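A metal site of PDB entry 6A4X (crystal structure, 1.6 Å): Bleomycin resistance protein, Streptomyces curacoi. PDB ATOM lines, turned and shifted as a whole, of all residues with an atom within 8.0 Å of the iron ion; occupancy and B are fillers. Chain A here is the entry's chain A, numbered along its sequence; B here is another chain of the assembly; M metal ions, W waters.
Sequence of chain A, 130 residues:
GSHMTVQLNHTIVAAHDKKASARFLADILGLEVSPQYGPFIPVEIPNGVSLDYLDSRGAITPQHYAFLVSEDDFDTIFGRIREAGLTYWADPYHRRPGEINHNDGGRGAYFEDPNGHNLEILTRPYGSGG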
ATOM      1  N   HIS A  64       6.390   6.746  15.237  1.00  0.00           N
ATOM      2  CA  HIS A  64       6.445   6.839  16.699  1.00  0.00           C
ATOM      3  C   HIS A  64       7.871   7.208  17.096  1.00  0.00           C
ATOM      4  O   HIS A  64       8.810   6.486  16.766  1.00  0.00           O
ATOM      5  CB  HIS A  64       6.041   5.520  17.360  1.00  0.00           C
ATOM      6  CG  HIS A  64       6.041   5.580  18.865  1.00  0.00           C
ATOM      7  ND1 HIS A  64       5.284   6.487  19.559  1.00  0.00           N
ATOM      8  CD2 HIS A  64       6.730   4.868  19.791  1.00  0.00           C
ATOM      9  CE1 HIS A  64       5.480   6.325  20.861  1.00  0.00           C
ATOM     10  NE2 HIS A  64       6.356   5.353  21.028  1.00  0.00           N
ATOM     11  N   TYR A  65       8.016   8.308  17.817  1.00  0.00           N
ATOM     12  CA  TYR A  65       9.320   8.781  18.279  1.00  0.00           C
ATOM     13  C   TYR A  65       9.221   8.994  19.785  1.00  0.00           C
ATOM     14  O   TYR A  65       8.438   9.834  20.239  1.00  0.00           O
ATOM     15  CB  TYR A  65       9.738  10.071  17.570  1.00  0.00           C
ATOM     16  CG  TYR A  65       9.707   9.948  16.060  1.00  0.00           C
ATOM     17  CD1 TYR A  65      10.650   9.170  15.393  1.00  0.00           C
ATOM     18  CD2 TYR A  65       8.732  10.600  15.301  1.00  0.00           C
ATOM     19  CE1 TYR A  65      10.622   9.041  14.007  1.00  0.00           C
ATOM     20  CE2 TYR A  65       8.694  10.481  13.914  1.00  0.00           C
ATOM     21  CZ  TYR A  65       9.650   9.698  13.277  1.00  0.00           C
ATOM     22  OH  TYR A  65       9.633   9.561  11.901  1.00  0.00           O
ATOM     23  N   ALA A  66      10.002   8.238  20.535  1.00  0.00           N
ATOM     24  CA  ALA A  66       9.946   8.268  21.991  1.00  0.00           C
ATOM     25  C   ALA A  66      11.250   8.819  22.540  1.00  0.00           C
ATOM     26  O   ALA A  66      12.328   8.361  22.154  1.00  0.00           O
ATOM     27  CB  ALA A  66       9.692   6.882  22.567  1.00  0.00           C
ATOM     28  N   PHE A  67      11.152   9.763  23.462  1.00  0.00           N
ATOM     29  CA  PHE A  67      12.315  10.472  23.985  1.00  0.00           C
ATOM     30  C   PHE A  67      12.446  10.191  25.461  1.00  0.00           C
ATOM     31  O   PHE A  67      11.483  10.366  26.218  1.00  0.00           O
ATOM     32  CB  PHE A  67      12.182  11.982  23.734  1.00  0.00           C
ATOM     33  CG  PHE A  67      12.105  12.330  22.290  1.00  0.00           C
ATOM     34  CD1 PHE A  67      13.268  12.558  21.555  1.00  0.00           C
ATOM     35  CD2 PHE A  67      10.890  12.370  21.636  1.00  0.00           C
ATOM     36  CE1 PHE A  67      13.210  12.844  20.204  1.00  0.00           C
ATOM     37  CE2 PHE A  67      10.820  12.662  20.264  1.00  0.00           C
ATOM     38  CZ  PHE A  67      11.986  12.895  19.558  1.00  0.00           C
ATOM     39  N   PRO A  92      -0.508   4.515  24.811  1.00  0.00           N
ATOM     40  CA  PRO A  92      -0.288   4.639  23.358  1.00  0.00           C
ATOM     41  C   PRO A  92      -1.553   4.513  22.537  1.00  0.00           C
ATOM     42  O   PRO A  92      -1.549   4.938  21.377  1.00  0.00           O
ATOM     43  CB  PRO A  92       0.697   3.494  23.055  1.00  0.00           C
ATOM     44  CG  PRO A  92       0.476   2.505  24.155  1.00  0.00           C
ATOM     45  CD  PRO A  92       0.176   3.335  25.378  1.00  0.00           C
ATOM     46  N   ASN A 103       5.286   4.383  34.054  1.00  0.00           N
ATOM     47  CA  ASN A 103       5.980   3.161  33.675  1.00  0.00           C
ATOM     48  C   ASN A 103       7.355   3.101  34.326  1.00  0.00           C
ATOM     49  O   ASN A 103       8.102   4.087  34.297  1.00  0.00           O
ATOM     50  CB  ASN A 103       6.150   3.058  32.160  1.00  0.00           C
ATOM     51  CG  ASN A 103       4.823   2.920  31.430  1.00  0.00           C
ATOM     52  OD1 ASN A 103       3.804   2.572  32.019  1.00  0.00           O
ATOM     53  ND2 ASN A 103       4.859   3.162  30.118  1.00  0.00           N
ATOM     54  N   ALA A 109       4.125  10.265  28.834  1.00  0.00           N
ATOM     55  CA  ALA A 109       2.898  10.695  28.197  1.00  0.00           C
ATOM     56  C   ALA A 109       3.091  10.657  26.697  1.00  0.00           C
ATOM     57  O   ALA A 109       4.215  10.707  26.196  1.00  0.00           O
ATOM     58  CB  ALA A 109       2.486  12.105  28.641  1.00  0.00           C
ATOM     59  N   TYR A 110       1.969  10.586  25.993  1.00  0.00           N
ATOM     60  CA  TYR A 110       1.945  10.555  24.536  1.00  0.00           C
ATOM     61  C   TYR A 110       1.216  11.795  24.014  1.00  0.00           C
ATOM     62  O   TYR A 110       0.242  12.247  24.626  1.00  0.00           O
ATOM     63  CB  TYR A 110       1.225   9.307  24.009  1.00  0.00           C
ATOM     64  CG  TYR A 110       1.860   7.993  24.413  1.00  0.00           C
ATOM     65  CD1 TYR A 110       2.681   7.296  23.538  1.00  0.00           C
ATOM     66  CD2 TYR A 110       1.613   7.454  25.673  1.00  0.00           C
ATOM     67  CE1 TYR A 110       3.254   6.096  23.906  1.00  0.00           C
ATOM     68  CE2 TYR A 110       2.196   6.247  26.051  1.00  0.00           C
ATOM     69  CZ  TYR A 110       3.016   5.587  25.159  1.00  0.00           C
ATOM     70  OH  TYR A 110       3.580   4.390  25.537  1.00  0.00           O
ATOM     71  N   ASN A 118       3.277  10.152  16.465  1.00  0.00           N
ATOM     72  CA  ASN A 118       3.018   9.845  17.866  1.00  0.00           C
ATOM     73  C   ASN A 118       4.291  10.113  18.638  1.00  0.00           C
ATOM     74  O   ASN A 118       5.262   9.352  18.528  1.00  0.00           O
ATOM     75  CB  ASN A 118       2.577   8.394  18.014  1.00  0.00           C
ATOM     76  CG  ASN A 118       1.230   8.144  17.390  1.00  0.00           C
ATOM     77  OD1 ASN A 118       0.213   8.662  17.871  1.00  0.00           O
ATOM     78  ND2 ASN A 118       1.204   7.353  16.319  1.00  0.00           N
ATOM     79  N   LEU A 119       4.292  11.176  19.433  1.00  0.00           N
ATOM     80  CA  LEU A 119       5.447  11.529  20.222  1.00  0.00           C
ATOM     81  C   LEU A 119       5.238  11.044  21.652  1.00  0.00           C
ATOM     82  O   LEU A 119       4.130  11.114  22.190  1.00  0.00           O
ATOM     83  CB  LEU A 119       5.691  13.036  20.207  1.00  0.00           C
ATOM     84  CG  LEU A 119       5.804  13.648  18.804  1.00  0.00           C
ATOM     85  CD1 LEU A 119       6.028  15.133  18.888  1.00  0.00           C
ATOM     86  CD2 LEU A 119       6.936  12.988  18.010  1.00  0.00           C
ATOM     87  N   GLU A 120       6.299  10.525  22.253  1.00  0.00           N
ATOM     88  CA  GLU A 120       6.232   9.994  23.605  1.00  0.00           C
ATOM     89  C   GLU A 120       7.402  10.533  24.406  1.00  0.00           C
ATOM     90  O   GLU A 120       8.526  10.632  23.896  1.00  0.00           O
ATOM     91  CB  GLU A 120       6.265   8.472  23.582  1.00  0.00           C
ATOM     92  CG  GLU A 120       6.301   7.826  24.966  1.00  0.00           C
ATOM     93  CD  GLU A 120       6.511   6.326  24.899  1.00  0.00           C
ATOM     94  OE1 GLU A 120       6.714   5.800  23.771  1.00  0.00           O
ATOM     95  OE2 GLU A 120       6.482   5.678  25.962  1.00  0.00           O
ATOM     96  N   ILE A 121       7.149  10.881  25.667  1.00  0.00           N
ATOM     97  CA  ILE A 121       8.228  11.170  26.600  1.00  0.00           C
ATOM     98  C   ILE A 121       8.141  10.170  27.738  1.00  0.00           C
ATOM     99  O   ILE A 121       7.064   9.702  28.081  1.00  0.00           O
ATOM    100  CB  ILE A 121       8.196  12.627  27.117  1.00  0.00           C
ATOM    101  CG1 ILE A 121       6.824  12.987  27.688  1.00  0.00           C
ATOM    102  CG2 ILE A 121       8.606  13.590  25.991  1.00  0.00           C
ATOM    103  CD1 ILE A 121       6.785  14.369  28.343  1.00  0.00           C
ATOM    104  N   LEU A 122       9.303   9.763  28.235  1.00  0.00           N
ATOM    105  CA  LEU A 122       9.410   8.779  29.298  1.00  0.00           C
ATOM    106  C   LEU A 122      10.646   9.152  30.084  1.00  0.00           C
ATOM    107  O   LEU A 122      11.572   9.751  29.527  1.00  0.00           O
ATOM    108  CB  LEU A 122       9.511   7.351  28.767  1.00  0.00           C
ATOM    109  CG  LEU A 122      10.637   7.047  27.761  1.00  0.00           C
ATOM    110  CD1 LEU A 122      11.181   5.656  27.985  1.00  0.00           C
ATOM    111  CD2 LEU A 122      10.134   7.189  26.313  1.00  0.00           C
ATOM    112  N   TYR A 126      11.972   1.477  29.263  1.00  0.00           N
ATOM    113  CA  TYR A 126      11.052   0.329  29.301  1.00  0.00           C
ATOM    114  C   TYR A 126      11.712  -0.890  29.930  1.00  0.00           C
ATOM    115  O   TYR A 126      12.728  -1.360  29.430  1.00  0.00           O
ATOM    116  CB  TYR A 126      10.585  -0.041  27.888  1.00  0.00           C
ATOM    117  CG  TYR A 126       9.633   0.891  27.204  1.00  0.00           C
ATOM    118  CD1 TYR A 126       9.175   2.042  27.838  1.00  0.00           C
ATOM    119  CD2 TYR A 126       9.181   0.608  25.925  1.00  0.00           C
ATOM    120  CE1 TYR A 126       8.295   2.898  27.181  1.00  0.00           C
ATOM    121  CE2 TYR A 126       8.301   1.454  25.271  1.00  0.00           C
ATOM    122  CZ  TYR A 126       7.864   2.597  25.914  1.00  0.00           C
ATOM    123  OH  TYR A 126       6.984   3.433  25.262  1.00  0.00           O
ATOM    124  N   ASN B   9      14.943   7.589  22.368  1.00  0.00           N
ATOM    125  CA  ASN B   9      15.011   6.282  23.028  1.00  0.00           C
ATOM    126  C   ASN B   9      14.537   5.129  22.147  1.00  0.00           C
ATOM    127  O   ASN B   9      15.130   4.044  22.214  1.00  0.00           O
ATOM    128  CB  ASN B   9      14.183   6.307  24.322  1.00  0.00           C
ATOM    129  CG  ASN B   9      14.306   5.026  25.114  1.00  0.00           C
ATOM    130  OD1 ASN B   9      15.276   4.818  25.848  1.00  0.00           O
ATOM    131  ND2 ASN B   9      13.320   4.135  24.956  1.00  0.00           N
ATOM    132  N   HIS B  10      13.472   5.318  21.366  1.00  0.00           N
ATOM    133  CA  HIS B  10      13.084   4.266  20.426  1.00  0.00           C
ATOM    134  C   HIS B  10      12.174   4.835  19.347  1.00  0.00           C
ATOM    135  O   HIS B  10      11.603   5.909  19.485  1.00  0.00           O
ATOM    136  CB  HIS B  10      12.435   3.056  21.133  1.00  0.00           C
ATOM    137  CG  HIS B  10      11.161   3.350  21.881  1.00  0.00           C
ATOM    138  ND1 HIS B  10      11.146   3.760  23.196  1.00  0.00           N
ATOM    139  CD2 HIS B  10       9.862   3.220  21.505  1.00  0.00           C
ATOM    140  CE1 HIS B  10       9.883   3.884  23.596  1.00  0.00           C
ATOM    141  NE2 HIS B  10       9.097   3.581  22.583  1.00  0.00           N
ATOM    142  N   THR B  11      12.114   4.106  18.226  1.00  0.00           N
ATOM    143  CA  THR B  11      11.122   4.316  17.186  1.00  0.00           C
ATOM    144  C   THR B  11      10.606   2.943  16.794  1.00  0.00           C
ATOM    145  O   THR B  11      11.242   1.919  17.069  1.00  0.00           O
ATOM    146  CB  THR B  11      11.681   5.100  15.977  1.00  0.00           C
ATOM    147  OG1 THR B  11      10.606   5.450  15.082  1.00  0.00           O
ATOM    148  CG2 THR B  11      12.735   4.287  15.232  1.00  0.00           C
ATOM    149  N   ILE B  12       9.414   2.890  16.187  1.00  0.00           N
ATOM    150  CA  ILE B  12       8.808   1.626  15.783  1.00  0.00           C
ATOM    151  C   ILE B  12       9.090   1.398  14.301  1.00  0.00           C
ATOM    152  O   ILE B  12       8.949   2.331  13.498  1.00  0.00           O
ATOM    153  CB  ILE B  12       7.299   1.615  16.073  1.00  0.00           C
ATOM    154  CG1 ILE B  12       7.078   1.724  17.572  1.00  0.00           C
ATOM    155  CG2 ILE B  12       6.649   0.337  15.544  1.00  0.00           C
ATOM    156  CD1 ILE B  12       5.603   1.946  17.956  1.00  0.00           C
ATOM    157  N   PHE B  40       6.799  -5.978  20.498  1.00  0.00           N
ATOM    158  CA  PHE B  40       7.969  -5.460  19.787  1.00  0.00           C
ATOM    159  C   PHE B  40       9.148  -6.420  19.857  1.00  0.00           C
ATOM    160  O   PHE B  40       9.365  -7.085  20.876  1.00  0.00           O
ATOM    161  CB  PHE B  40       8.404  -4.114  20.357  1.00  0.00           C
ATOM    162  CG  PHE B  40       7.331  -3.066  20.319  1.00  0.00           C
ATOM    163  CD1 PHE B  40       6.982  -2.466  19.123  1.00  0.00           C
ATOM    164  CD2 PHE B  40       6.686  -2.678  21.482  1.00  0.00           C
ATOM    165  CE1 PHE B  40       5.999  -1.499  19.091  1.00  0.00           C
ATOM    166  CE2 PHE B  40       5.701  -1.712  21.441  1.00  0.00           C
ATOM    167  CZ  PHE B  40       5.362  -1.125  20.235  1.00  0.00           C
ATOM    168  N   ASP B  52      12.320  -0.737  17.217  1.00  0.00           N
ATOM    169  CA  ASP B  52      11.401  -1.707  17.805  1.00  0.00           C
ATOM    170  C   ASP B  52      10.491  -2.243  16.698  1.00  0.00           C
ATOM    171  O   ASP B  52       9.589  -1.542  16.238  1.00  0.00           O
ATOM    172  CB  ASP B  52      10.595  -1.073  18.926  1.00  0.00           C
ATOM    173  CG  ASP B  52      11.453  -0.671  20.127  1.00  0.00           C
ATOM    174  OD1 ASP B  52      12.665  -0.940  20.130  1.00  0.00           O
ATOM    175  OD2 ASP B  52      10.888  -0.081  21.067  1.00  0.00           O
HETATM  176 FE    FE M   1       6.765   4.011  22.907  1.00  0.00          FE
HETATM  177  O   HOH W   1       6.613   1.954  21.985  1.00  0.00           O
HETATM  178  O   HOH W   2       5.135   3.234  23.975  1.00  0.00           O
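The iron ion is bound by OE1 of Glu 120 (2.0 Å), water W2 (2.1 Å), water W1 (2.3 Å), NE2 of His 64 (2.3 Å), NE2 of His 10 of chain B (2.4 Å) and OH of Tyr 126 (2.4 Å).
Of the 20 residues printed, 4 come within 4 Å of the iron ion.
O of Tyr 65 is in hydrogen-bond range of N of Glu 120.
O of Asn 118 lies within hydrogen-bond range of ND1 of His 64 (3.0 Å).
The side-chain hydroxyl (OH) of Tyr 110 sits at hydrogen-bond distance from the side-chain carboxylate (OE2) of Glu 120.
ND1 of His 10 of chain B lies within hydrogen-bond range of ND2 of Asn 9 of chain B, at 2.8 Å.
The backbone carbonyl oxygen (O) of His 64 is in hydrogen-bond range of the side-chain hydroxyl (OG1) of Thr 11 of chain B, 2.7 Å away.
The backbone carbonyl oxygen (O) of Glu 120 is in hydrogen-bond range of the backbone NH (N) of Phe 67.
The backbone NH (N) of Ala 66 is in hydrogen-bond range of the backbone carbonyl oxygen (O) of His 10 of chain B, at 3.0 Å.
Water W2 bridges OH of Tyr 110 (2.5 Å) and OE2 of Glu 120 (3.4 Å).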
